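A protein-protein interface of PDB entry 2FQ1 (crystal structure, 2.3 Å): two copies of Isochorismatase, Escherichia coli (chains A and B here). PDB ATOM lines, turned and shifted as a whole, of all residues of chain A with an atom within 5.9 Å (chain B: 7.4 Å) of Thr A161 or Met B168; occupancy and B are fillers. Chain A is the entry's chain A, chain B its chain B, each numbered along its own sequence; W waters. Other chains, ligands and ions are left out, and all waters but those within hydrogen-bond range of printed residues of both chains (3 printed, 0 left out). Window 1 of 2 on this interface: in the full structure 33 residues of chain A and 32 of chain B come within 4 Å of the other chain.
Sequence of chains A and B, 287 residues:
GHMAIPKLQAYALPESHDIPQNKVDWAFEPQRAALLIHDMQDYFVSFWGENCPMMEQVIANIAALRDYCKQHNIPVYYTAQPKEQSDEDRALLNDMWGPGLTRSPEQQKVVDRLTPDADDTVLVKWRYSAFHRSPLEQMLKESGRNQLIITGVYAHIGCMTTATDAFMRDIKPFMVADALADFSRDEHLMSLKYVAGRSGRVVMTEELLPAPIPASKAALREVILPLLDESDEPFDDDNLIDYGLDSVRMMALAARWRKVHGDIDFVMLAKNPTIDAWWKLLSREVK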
ATOM      1  N   ARG A 127     -14.175   9.999  11.808  1.00  0.00           N
ATOM      2  CA  ARG A 127     -15.221   9.095  12.268  1.00  0.00           C
ATOM      3  C   ARG A 127     -15.312   7.897  11.308  1.00  0.00           C
ATOM      4  O   ARG A 127     -14.735   7.926  10.213  1.00  0.00           O
ATOM      5  CB  ARG A 127     -16.579   9.841  12.333  1.00  0.00           C
ATOM      6  CG  ARG A 127     -16.647  11.040  13.298  1.00  0.00           C
ATOM      7  CD  ARG A 127     -16.526  10.583  14.766  1.00  0.00           C
ATOM      8  NE  ARG A 127     -16.713  11.659  15.736  1.00  0.00           N
ATOM      9  CZ  ARG A 127     -15.720  12.357  16.293  1.00  0.00           C
ATOM     10  NH1 ARG A 127     -14.444  12.090  16.002  1.00  0.00           N
ATOM     11  NH2 ARG A 127     -16.001  13.313  17.163  1.00  0.00           N
ATOM     12  N   TYR A 128     -16.042   6.853  11.707  1.00  0.00           N
ATOM     13  CA  TYR A 128     -16.230   5.660  10.855  1.00  0.00           C
ATOM     14  C   TYR A 128     -16.666   5.981   9.424  1.00  0.00           C
ATOM     15  O   TYR A 128     -16.169   5.381   8.489  1.00  0.00           O
ATOM     16  CB  TYR A 128     -17.237   4.675  11.459  1.00  0.00           C
ATOM     17  CG  TYR A 128     -16.908   4.093  12.828  1.00  0.00           C
ATOM     18  CD1 TYR A 128     -15.584   3.889  13.252  1.00  0.00           C
ATOM     19  CD2 TYR A 128     -17.944   3.694  13.683  1.00  0.00           C
ATOM     20  CE1 TYR A 128     -15.301   3.322  14.540  1.00  0.00           C
ATOM     21  CE2 TYR A 128     -17.675   3.122  14.948  1.00  0.00           C
ATOM     22  CZ  TYR A 128     -16.355   2.943  15.359  1.00  0.00           C
ATOM     23  OH  TYR A 128     -16.125   2.379  16.588  1.00  0.00           O
ATOM     24  N   SER A 129     -17.601   6.918   9.271  1.00  0.00           N
ATOM     25  CA  SER A 129     -18.098   7.312   7.972  1.00  0.00           C
ATOM     26  C   SER A 129     -17.210   8.373   7.347  1.00  0.00           C
ATOM     27  O   SER A 129     -16.981   9.430   7.951  1.00  0.00           O
ATOM     28  CB  SER A 129     -19.514   7.868   8.108  1.00  0.00           C
ATOM     29  OG  SER A 129     -19.948   8.402   6.881  1.00  0.00           O
ATOM     30  N   HIS A 132     -18.624  11.908   7.403  1.00  0.00           N
ATOM     31  CA  HIS A 132     -18.668  12.727   8.630  1.00  0.00           C
ATOM     32  C   HIS A 132     -17.481  13.681   8.735  1.00  0.00           C
ATOM     33  O   HIS A 132     -16.317  13.264   8.612  1.00  0.00           O
ATOM     34  CB  HIS A 132     -18.780  11.853   9.894  1.00  0.00           C
ATOM     35  CG  HIS A 132     -20.190  11.507  10.251  1.00  0.00           C
ATOM     36  ND1 HIS A 132     -20.758  11.845  11.462  1.00  0.00           N
ATOM     37  CD2 HIS A 132     -21.163  10.889   9.537  1.00  0.00           C
ATOM     38  CE1 HIS A 132     -22.011  11.421  11.487  1.00  0.00           C
ATOM     39  NE2 HIS A 132     -22.280  10.837  10.333  1.00  0.00           N
ATOM     40  N   ARG A 133     -17.795  14.962   8.945  1.00  0.00           N
ATOM     41  CA  ARG A 133     -16.790  16.017   9.156  1.00  0.00           C
ATOM     42  C   ARG A 133     -15.812  16.128   8.002  1.00  0.00           C
ATOM     43  O   ARG A 133     -14.660  16.541   8.183  1.00  0.00           O
ATOM     44  CB  ARG A 133     -16.048  15.830  10.490  1.00  0.00           C
ATOM     45  CG  ARG A 133     -16.945  16.007  11.711  1.00  0.00           C
ATOM     46  CD  ARG A 133     -16.318  15.495  13.000  1.00  0.00           C
ATOM     47  NE  ARG A 133     -17.369  15.152  13.953  1.00  0.00           N
ATOM     48  CZ  ARG A 133     -17.371  15.472  15.249  1.00  0.00           C
ATOM     49  NH1 ARG A 133     -16.364  16.166  15.784  1.00  0.00           N
ATOM     50  NH2 ARG A 133     -18.400  15.110  16.014  1.00  0.00           N
ATOM     51  N   ALA A 155     -13.594  -3.924   7.040  1.00  0.00           N
ATOM     52  CA  ALA A 155     -14.865  -4.120   6.328  1.00  0.00           C
ATOM     53  C   ALA A 155     -16.130  -3.750   7.101  1.00  0.00           C
ATOM     54  O   ALA A 155     -16.905  -2.909   6.641  1.00  0.00           O
ATOM     55  CB  ALA A 155     -14.965  -5.548   5.779  1.00  0.00           C
ATOM     56  N   HIS A 156     -16.347  -4.371   8.260  1.00  0.00           N
ATOM     57  CA  HIS A 156     -17.609  -4.204   9.002  1.00  0.00           C
ATOM     58  C   HIS A 156     -17.753  -2.890   9.797  1.00  0.00           C
ATOM     59  O   HIS A 156     -18.856  -2.567  10.254  1.00  0.00           O
ATOM     60  CB  HIS A 156     -17.879  -5.426   9.902  1.00  0.00           C
ATOM     61  CG  HIS A 156     -17.159  -5.390  11.215  1.00  0.00           C
ATOM     62  ND1 HIS A 156     -15.802  -5.621  11.330  1.00  0.00           N
ATOM     63  CD2 HIS A 156     -17.609  -5.162  12.470  1.00  0.00           C
ATOM     64  CE1 HIS A 156     -15.444  -5.507  12.592  1.00  0.00           C
ATOM     65  NE2 HIS A 156     -16.520  -5.216  13.303  1.00  0.00           N
ATOM     66  N   ILE A 157     -16.651  -2.152   9.979  1.00  0.00           N
ATOM     67  CA  ILE A 157     -16.666  -0.898  10.757  1.00  0.00           C
ATOM     68  C   ILE A 157     -16.786   0.348   9.838  1.00  0.00           C
ATOM     69  O   ILE A 157     -17.881   0.684   9.372  1.00  0.00           O
ATOM     70  CB  ILE A 157     -15.453  -0.815  11.769  1.00  0.00           C
ATOM     71  CG1 ILE A 157     -15.274  -2.142  12.504  1.00  0.00           C
ATOM     72  CG2 ILE A 157     -15.632   0.331  12.765  1.00  0.00           C
ATOM     73  CD1 ILE A 157     -13.971  -2.259  13.367  1.00  0.00           C
ATOM     74  N   GLY A 158     -15.675   1.015   9.552  1.00  0.00           N
ATOM     75  CA  GLY A 158     -15.697   2.188   8.694  1.00  0.00           C
ATOM     76  C   GLY A 158     -16.158   1.993   7.250  1.00  0.00           C
ATOM     77  O   GLY A 158     -16.833   2.861   6.686  1.00  0.00           O
ATOM     78  N   CYS A 159     -15.786   0.877   6.631  1.00  0.00           N
ATOM     79  CA  CYS A 159     -16.187   0.648   5.252  1.00  0.00           C
ATOM     80  C   CYS A 159     -17.689   0.456   5.152  1.00  0.00           C
ATOM     81  O   CYS A 159     -18.336   1.005   4.254  1.00  0.00           O
ATOM     82  CB  CYS A 159     -15.455  -0.554   4.633  1.00  0.00           C
ATOM     83  SG  CYS A 159     -13.677  -0.350   4.512  1.00  0.00           S
ATOM     84  N   MET A 160     -18.235  -0.351   6.057  1.00  0.00           N
ATOM     85  CA  MET A 160     -19.668  -0.663   6.050  1.00  0.00           C
ATOM     86  C   MET A 160     -20.521   0.549   6.450  1.00  0.00           C
ATOM     87  O   MET A 160     -21.591   0.751   5.894  1.00  0.00           O
ATOM     88  CB  MET A 160     -19.968  -1.858   6.946  1.00  0.00           C
ATOM     89  CG  MET A 160     -21.360  -2.402   6.774  1.00  0.00           C
ATOM     90  SD  MET A 160     -21.727  -3.766   7.874  1.00  0.00           S
ATOM     91  CE  MET A 160     -22.169  -2.896   9.361  1.00  0.00           C
ATOM     92  N   THR A 161     -20.019   1.354   7.389  1.00  0.00           N
ATOM     93  CA  THR A 161     -20.653   2.605   7.820  1.00  0.00           C
ATOM     94  C   THR A 161     -20.702   3.671   6.717  1.00  0.00           C
ATOM     95  O   THR A 161     -21.740   4.287   6.486  1.00  0.00           O
ATOM     96  CB  THR A 161     -19.971   3.160   9.093  1.00  0.00           C
ATOM     97  OG1 THR A 161     -20.079   2.167  10.115  1.00  0.00           O
ATOM     98  CG2 THR A 161     -20.657   4.439   9.581  1.00  0.00           C
ATOM     99  N   THR A 162     -19.581   3.867   6.036  1.00  0.00           N
ATOM    100  CA  THR A 162     -19.514   4.727   4.864  1.00  0.00           C
ATOM    101  C   THR A 162     -20.519   4.276   3.783  1.00  0.00           C
ATOM    102  O   THR A 162     -21.161   5.121   3.137  1.00  0.00           O
ATOM    103  CB  THR A 162     -18.088   4.718   4.293  1.00  0.00           C
ATOM    104  OG1 THR A 162     -17.173   5.193   5.293  1.00  0.00           O
ATOM    105  CG2 THR A 162     -17.982   5.568   3.024  1.00  0.00           C
ATOM    106  N   ALA A 163     -20.652   2.958   3.600  1.00  0.00           N
ATOM    107  CA  ALA A 163     -21.585   2.375   2.621  1.00  0.00           C
ATOM    108  C   ALA A 163     -23.016   2.785   2.944  1.00  0.00           C
ATOM    109  O   ALA A 163     -23.730   3.301   2.083  1.00  0.00           O
ATOM    110  CB  ALA A 163     -21.458   0.824   2.578  1.00  0.00           C
ATOM    111  N   THR A 164     -23.423   2.573   4.198  1.00  0.00           N
ATOM    112  CA  THR A 164     -24.769   2.921   4.648  1.00  0.00           C
ATOM    113  C   THR A 164     -24.977   4.430   4.539  1.00  0.00           C
ATOM    114  O   THR A 164     -25.998   4.893   4.030  1.00  0.00           O
ATOM    115  CB  THR A 164     -25.034   2.364   6.072  1.00  0.00           C
ATOM    116  OG1 THR A 164     -24.826   0.953   6.048  1.00  0.00           O
ATOM    117  CG2 THR A 164     -26.470   2.615   6.539  1.00  0.00           C
ATOM    118  N   ASP A 165     -23.992   5.188   5.005  1.00  0.00           N
ATOM    119  CA  ASP A 165     -24.043   6.642   4.931  1.00  0.00           C
ATOM    120  C   ASP A 165     -24.189   7.176   3.497  1.00  0.00           C
ATOM    121  O   ASP A 165     -25.073   8.004   3.234  1.00  0.00           O
ATOM    122  CB  ASP A 165     -22.825   7.249   5.615  1.00  0.00           C
ATOM    123  CG  ASP A 165     -23.097   8.612   6.132  1.00  0.00           C
ATOM    124  OD1 ASP A 165     -24.221   9.106   5.918  1.00  0.00           O
ATOM    125  OD2 ASP A 165     -22.213   9.188   6.772  1.00  0.00           O
ATOM    126  N   ALA A 166     -23.329   6.710   2.584  1.00  0.00           N
ATOM    127  CA  ALA A 166     -23.471   6.977   1.130  1.00  0.00           C
ATOM    128  C   ALA A 166     -24.910   6.753   0.612  1.00  0.00           C
ATOM    129  O   ALA A 166     -25.552   7.684   0.149  1.00  0.00           O
ATOM    130  CB  ALA A 166     -22.441   6.118   0.314  1.00  0.00           C
ATOM    131  N   SER B 129     -30.940   6.388   9.830  1.00  0.00           N
ATOM    132  CA  SER B 129     -30.518   7.160  10.977  1.00  0.00           C
ATOM    133  C   SER B 129     -31.522   8.255  11.324  1.00  0.00           C
ATOM    134  O   SER B 129     -31.950   9.025  10.450  1.00  0.00           O
ATOM    135  CB  SER B 129     -29.176   7.766  10.695  1.00  0.00           C
ATOM    136  OG  SER B 129     -28.760   8.516  11.796  1.00  0.00           O
ATOM    137  N   HIS B 132     -30.505  11.974  10.380  1.00  0.00           N
ATOM    138  CA  HIS B 132     -30.450  12.449   8.990  1.00  0.00           C
ATOM    139  C   HIS B 132     -31.715  13.219   8.603  1.00  0.00           C
ATOM    140  O   HIS B 132     -32.831  12.735   8.820  1.00  0.00           O
ATOM    141  CB  HIS B 132     -30.265  11.269   8.028  1.00  0.00           C
ATOM    142  CG  HIS B 132     -28.837  10.975   7.692  1.00  0.00           C
ATOM    143  ND1 HIS B 132     -28.362  10.986   6.396  1.00  0.00           N
ATOM    144  CD2 HIS B 132     -27.778  10.664   8.478  1.00  0.00           C
ATOM    145  CE1 HIS B 132     -27.073  10.687   6.400  1.00  0.00           C
ATOM    146  NE2 HIS B 132     -26.693  10.493   7.649  1.00  0.00           N
ATOM    147  N   GLU B 137     -30.054  15.998  16.425  1.00  0.00           N
ATOM    148  CA  GLU B 137     -28.777  16.350  17.061  1.00  0.00           C
ATOM    149  C   GLU B 137     -28.804  17.715  17.733  1.00  0.00           C
ATOM    150  O   GLU B 137     -28.308  17.867  18.847  1.00  0.00           O
ATOM    151  CB  GLU B 137     -27.629  16.320  16.052  1.00  0.00           C
ATOM    152  CG  GLU B 137     -26.268  16.626  16.708  1.00  0.00           C
ATOM    153  CD  GLU B 137     -25.103  16.544  15.746  1.00  0.00           C
ATOM    154  OE1 GLU B 137     -23.946  16.682  16.196  1.00  0.00           O
ATOM    155  OE2 GLU B 137     -25.347  16.335  14.545  1.00  0.00           O
ATOM    156  N   THR B 161     -28.000   1.788  13.007  1.00  0.00           N
ATOM    157  CA  THR B 161     -27.476   2.953  12.285  1.00  0.00           C
ATOM    158  C   THR B 161     -27.590   4.223  13.108  1.00  0.00           C
ATOM    159  O   THR B 161     -26.640   4.996  13.170  1.00  0.00           O
ATOM    160  CB  THR B 161     -28.140   3.150  10.898  1.00  0.00           C
ATOM    161  OG1 THR B 161     -28.065   1.924  10.160  1.00  0.00           O
ATOM    162  CG2 THR B 161     -27.435   4.279  10.080  1.00  0.00           C
ATOM    163  N   THR B 162     -28.744   4.428  13.740  1.00  0.00           N
ATOM    164  CA  THR B 162     -28.953   5.571  14.640  1.00  0.00           C
ATOM    165  C   THR B 162     -27.940   5.588  15.803  1.00  0.00           C
ATOM    166  O   THR B 162     -27.388   6.645  16.114  1.00  0.00           O
ATOM    167  CB  THR B 162     -30.405   5.586  15.145  1.00  0.00           C
ATOM    168  OG1 THR B 162     -31.287   5.852  14.036  1.00  0.00           O
ATOM    169  CG2 THR B 162     -30.614   6.636  16.207  1.00  0.00           C
ATOM    170  N   ALA B 163     -27.683   4.420  16.406  1.00  0.00           N
ATOM    171  CA  ALA B 163     -26.669   4.245  17.468  1.00  0.00           C
ATOM    172  C   ALA B 163     -25.267   4.634  17.035  1.00  0.00           C
ATOM    173  O   ALA B 163     -24.587   5.400  17.722  1.00  0.00           O
ATOM    174  CB  ALA B 163     -26.674   2.791  17.987  1.00  0.00           C
ATOM    175  N   THR B 164     -24.838   4.095  15.901  1.00  0.00           N
ATOM    176  CA  THR B 164     -23.551   4.436  15.298  1.00  0.00           C
ATOM    177  C   THR B 164     -23.485   5.922  14.930  1.00  0.00           C
ATOM    178  O   THR B 164     -22.486   6.589  15.213  1.00  0.00           O
ATOM    179  CB  THR B 164     -23.244   3.522  14.071  1.00  0.00           C
ATOM    180  OG1 THR B 164     -23.483   2.158  14.439  1.00  0.00           O
ATOM    181  CG2 THR B 164     -21.802   3.654  13.614  1.00  0.00           C
ATOM    182  N   ASP B 165     -24.556   6.450  14.341  1.00  0.00           N
ATOM    183  CA  ASP B 165     -24.595   7.871  13.990  1.00  0.00           C
ATOM    184  C   ASP B 165     -24.560   8.775  15.246  1.00  0.00           C
ATOM    185  O   ASP B 165     -23.931   9.833  15.231  1.00  0.00           O
ATOM    186  CB  ASP B 165     -25.813   8.169  13.117  1.00  0.00           C
ATOM    187  CG  ASP B 165     -25.650   9.421  12.282  1.00  0.00           C
ATOM    188  OD1 ASP B 165     -24.616  10.112  12.433  1.00  0.00           O
ATOM    189  OD2 ASP B 165     -26.549   9.701  11.452  1.00  0.00           O
ATOM    190  N   ALA B 166     -25.240   8.350  16.319  1.00  0.00           N
ATOM    191  CA  ALA B 166     -25.198   9.036  17.608  1.00  0.00           C
ATOM    192  C   ALA B 166     -23.773   9.078  18.160  1.00  0.00           C
ATOM    193  O   ALA B 166     -23.288  10.121  18.561  1.00  0.00           O
ATOM    194  CB  ALA B 166     -26.138   8.335  18.626  1.00  0.00           C
ATOM    195  N   PHE B 167     -23.130   7.915  18.194  1.00  0.00           N
ATOM    196  CA  PHE B 167     -21.752   7.745  18.630  1.00  0.00           C
ATOM    197  C   PHE B 167     -20.824   8.675  17.854  1.00  0.00           C
ATOM    198  O   PHE B 167     -19.954   9.327  18.450  1.00  0.00           O
ATOM    199  CB  PHE B 167     -21.378   6.255  18.478  1.00  0.00           C
ATOM    200  CG  PHE B 167     -19.920   5.927  18.716  1.00  0.00           C
ATOM    201  CD1 PHE B 167     -19.377   5.936  19.998  1.00  0.00           C
ATOM    202  CD2 PHE B 167     -19.108   5.529  17.660  1.00  0.00           C
ATOM    203  CE1 PHE B 167     -18.030   5.609  20.214  1.00  0.00           C
ATOM    204  CE2 PHE B 167     -17.766   5.202  17.872  1.00  0.00           C
ATOM    205  CZ  PHE B 167     -17.226   5.247  19.156  1.00  0.00           C
ATOM    206  N   MET B 168     -21.027   8.763  16.535  1.00  0.00           N
ATOM    207  CA  MET B 168     -20.201   9.625  15.685  1.00  0.00           C
ATOM    208  C   MET B 168     -20.472  11.099  15.961  1.00  0.00           C
ATOM    209  O   MET B 168     -19.583  11.938  15.839  1.00  0.00           O
ATOM    210  CB  MET B 168     -20.419   9.323  14.200  1.00  0.00           C
ATOM    211  CG  MET B 168     -19.943   7.955  13.756  1.00  0.00           C
ATOM    212  SD  MET B 168     -19.873   7.825  11.979  1.00  0.00           S
ATOM    213  CE  MET B 168     -21.602   7.597  11.487  1.00  0.00           C
ATOM    214  N   ARG B 169     -21.710  11.411  16.322  1.00  0.00           N
ATOM    215  CA  ARG B 169     -22.090  12.784  16.680  1.00  0.00           C
ATOM    216  C   ARG B 169     -21.888  13.113  18.191  1.00  0.00           C
ATOM    217  O   ARG B 169     -22.435  14.104  18.692  1.00  0.00           O
ATOM    218  CB  ARG B 169     -23.526  13.046  16.227  1.00  0.00           C
ATOM    219  CG  ARG B 169     -23.711  13.061  14.689  1.00  0.00           C
ATOM    220  CD  ARG B 169     -25.166  12.831  14.330  1.00  0.00           C
ATOM    221  NE  ARG B 169     -25.385  12.503  12.909  1.00  0.00           N
ATOM    222  CZ  ARG B 169     -25.824  13.357  11.988  1.00  0.00           C
ATOM    223  NH1 ARG B 169     -26.110  14.608  12.317  1.00  0.00           N
ATOM    224  NH2 ARG B 169     -25.998  12.956  10.730  1.00  0.00           N
ATOM    225  N   ASP B 170     -21.098  12.284  18.891  1.00  0.00           N
ATOM    226  CA  ASP B 170     -20.737  12.450  20.335  1.00  0.00           C
ATOM    227  C   ASP B 170     -21.914  12.316  21.310  1.00  0.00           C
ATOM    228  O   ASP B 170     -21.980  13.000  22.328  1.00  0.00           O
ATOM    229  CB  ASP B 170     -19.972  13.758  20.568  1.00  0.00           C
ATOM    230  CG  ASP B 170     -18.902  13.983  19.542  1.00  0.00           C
ATOM    231  OD1 ASP B 170     -18.371  12.974  19.045  1.00  0.00           O
ATOM    232  OD2 ASP B 170     -18.589  15.150  19.229  1.00  0.00           O
ATOM    233  N   ILE B 171     -22.842  11.432  20.973  1.00  0.00           N
ATOM    234  CA  ILE B 171     -23.996  11.091  21.805  1.00  0.00           C
ATOM    235  C   ILE B 171     -23.838   9.608  22.193  1.00  0.00           C
ATOM    236  O   ILE B 171     -23.476   8.782  21.364  1.00  0.00           O
ATOM    237  CB  ILE B 171     -25.337  11.374  21.029  1.00  0.00           C
ATOM    238  CG1 ILE B 171     -25.440  12.871  20.684  1.00  0.00           C
ATOM    239  CG2 ILE B 171     -26.558  10.967  21.836  1.00  0.00           C
ATOM    240  CD1 ILE B 171     -26.314  13.189  19.469  1.00  0.00           C
ATOM    241  N   PRO B 173     -25.024   6.055  22.850  1.00  0.00           N
ATOM    242  CA  PRO B 173     -26.152   5.162  22.659  1.00  0.00           C
ATOM    243  C   PRO B 173     -26.245   4.104  23.771  1.00  0.00           C
ATOM    244  O   PRO B 173     -25.236   3.523  24.182  1.00  0.00           O
ATOM    245  CB  PRO B 173     -25.854   4.493  21.299  1.00  0.00           C
ATOM    246  CG  PRO B 173     -24.635   5.183  20.763  1.00  0.00           C
ATOM    247  CD  PRO B 173     -23.909   5.707  21.949  1.00  0.00           C
ATOM    248  N   TYR B 194     -22.578  -5.728  17.694  1.00  0.00           N
ATOM    249  CA  TYR B 194     -22.083  -4.563  16.973  1.00  0.00           C
ATOM    250  C   TYR B 194     -21.992  -3.325  17.862  1.00  0.00           C
ATOM    251  O   TYR B 194     -20.921  -2.766  18.027  1.00  0.00           O
ATOM    252  CB  TYR B 194     -22.938  -4.269  15.746  1.00  0.00           C
ATOM    253  CG  TYR B 194     -22.186  -3.440  14.734  1.00  0.00           C
ATOM    254  CD1 TYR B 194     -22.155  -2.032  14.817  1.00  0.00           C
ATOM    255  CD2 TYR B 194     -21.500  -4.058  13.692  1.00  0.00           C
ATOM    256  CE1 TYR B 194     -21.461  -1.281  13.880  1.00  0.00           C
ATOM    257  CE2 TYR B 194     -20.798  -3.324  12.767  1.00  0.00           C
ATOM    258  CZ  TYR B 194     -20.771  -1.947  12.866  1.00  0.00           C
ATOM    259  OH  TYR B 194     -20.056  -1.267  11.925  1.00  0.00           O
ATOM    260  N   SER B 199     -19.940   0.924  19.163  1.00  0.00           N
ATOM    261  CA  SER B 199     -20.664   2.201  19.218  1.00  0.00           C
ATOM    262  C   SER B 199     -21.330   2.597  20.546  1.00  0.00           C
ATOM    263  O   SER B 199     -21.642   3.771  20.745  1.00  0.00           O
ATOM    264  CB  SER B 199     -21.707   2.265  18.094  1.00  0.00           C
ATOM    265  OG  SER B 199     -22.807   1.432  18.427  1.00  0.00           O
HETATM  266  O   HOH W   1     -16.199  16.185  18.810  1.00  0.00           O
HETATM  267  O   HOH W   2     -19.837  13.634  13.094  1.00  0.00           O
HETATM  268  O   HOH W   3     -20.838  16.262  16.279  1.00  0.00           O
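Hydrophobic or aromatic side chains of chain B that line the printed part of chain A: His B132, Phe B167, Met B168 and Tyr B194.
Of the 17 printed residues of chain A, 10 touch a printed residue of chain B.
Hydrophobic or aromatic side chains of chain A within 4 Å of the printed part of chain B: Tyr A128, His A132, His A156 and Met A160.
Among the printed residues, 17 pairs touch across the chains.
Among the printed residues, Asp or Glu carboxylates within 4 Å of a Lys or Arg side-chain nitrogen of the other chain: Arg A127 with Asp B170 and Arg A133 with Asp B170.
His A132 touches Asp B165, and with the chains exchanged Asp A165 touches His B132.
Positions printed for both chains: 129, 132, 161, 162, 163, 164, 165 and 166.
Of the 17 pairs that touch across the chains among the printed residues, 2 have their exchanged pair printed and touching as well.
The backbone NH (N) of Ser A129 lies within hydrogen-bond range of the side-chain sulfur (SD) of Met B168 (3.6 Å).
O of His A156 lies within hydrogen-bond range of OH of Tyr B194.
OD1 of Asp B165 sits close to NE2 of His A132.
The guanidinium group of Arg A127 lies within hydrogen-bond range of the backbone carbonyl oxygen of Met B168.
OD1 of Asp B170 lies within salt-bridge range of NH2 of Arg A127.
NH2 of Arg A133 is in salt-bridge range of OD2 of Asp B170.
The guanidinium group (NH2) of Arg A133 is in hydrogen-bond range of the backbone carbonyl oxygen (O) of Met B168.
NE2 of His B132 sits close to OD1 of Asp A165, 3.3 Å away.
OE2 of Glu B137 lies within salt-bridge range of NH1 of Arg B169 (2.9 Å).
O of Ala A155 is in hydrogen-bond range of N of Met A160.
O of Ile A157 sits at hydrogen-bond distance from OG1 of Thr A161 (2.8 Å).
The side-chain carboxylate (OD1) of Asp B165 lies within salt-bridge range of the guanidinium group (NE) of Arg B169 (2.6 Å).
The side-chain hydroxyl of Thr A162 is in hydrogen-bond range of the backbone carbonyl oxygen of Tyr A128.
The side-chain carboxylate of Asp B165 sits at hydrogen-bond distance from the side-chain hydroxyl of Ser B129, at 2.5 Å.
Among the printed residues, merely in contact across the chains: His A132 with Met B168, Tyr A128 with Phe B167, Ile A157 with Tyr B194, Met A160 with Tyr B194, Thr A161 with Met B168, His A132 with Arg B169, Tyr A128 with Thr B164, Thr A161 with Tyr B194 and Tyr A128 with Met B168.
Water W2 lies within hydrogen-bond range of a ring nitrogen (ND1) of His A132 (2.6 Å), the guanidinium group of Arg A133 (3.0 Å) and the backbone carbonyl oxygen of Met B168 (3.2 Å).
Water W1 lies within hydrogen-bond range of the side-chain carboxylate of Asp B170, the guanidinium group of Arg A133 and the guanidinium group of Arg A127.
Water W3 lies within hydrogen-bond range of NH2 of Arg A133 and OE1 of Glu B137.
Of chain B, only Met B168 and Tyr B194 come within 4 Å of Thr A161.
Of the printed residues of chain B, Asp A165 touches His B132 (3.3 Å).
Of the printed residues of chain A, Arg B169 touches His A132 (3.8 Å).
Pro B173 touches none of the printed residues of chain A.
The nearest residue of chain B that does not touch Thr A161 is Thr B164 (4.2 Å).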
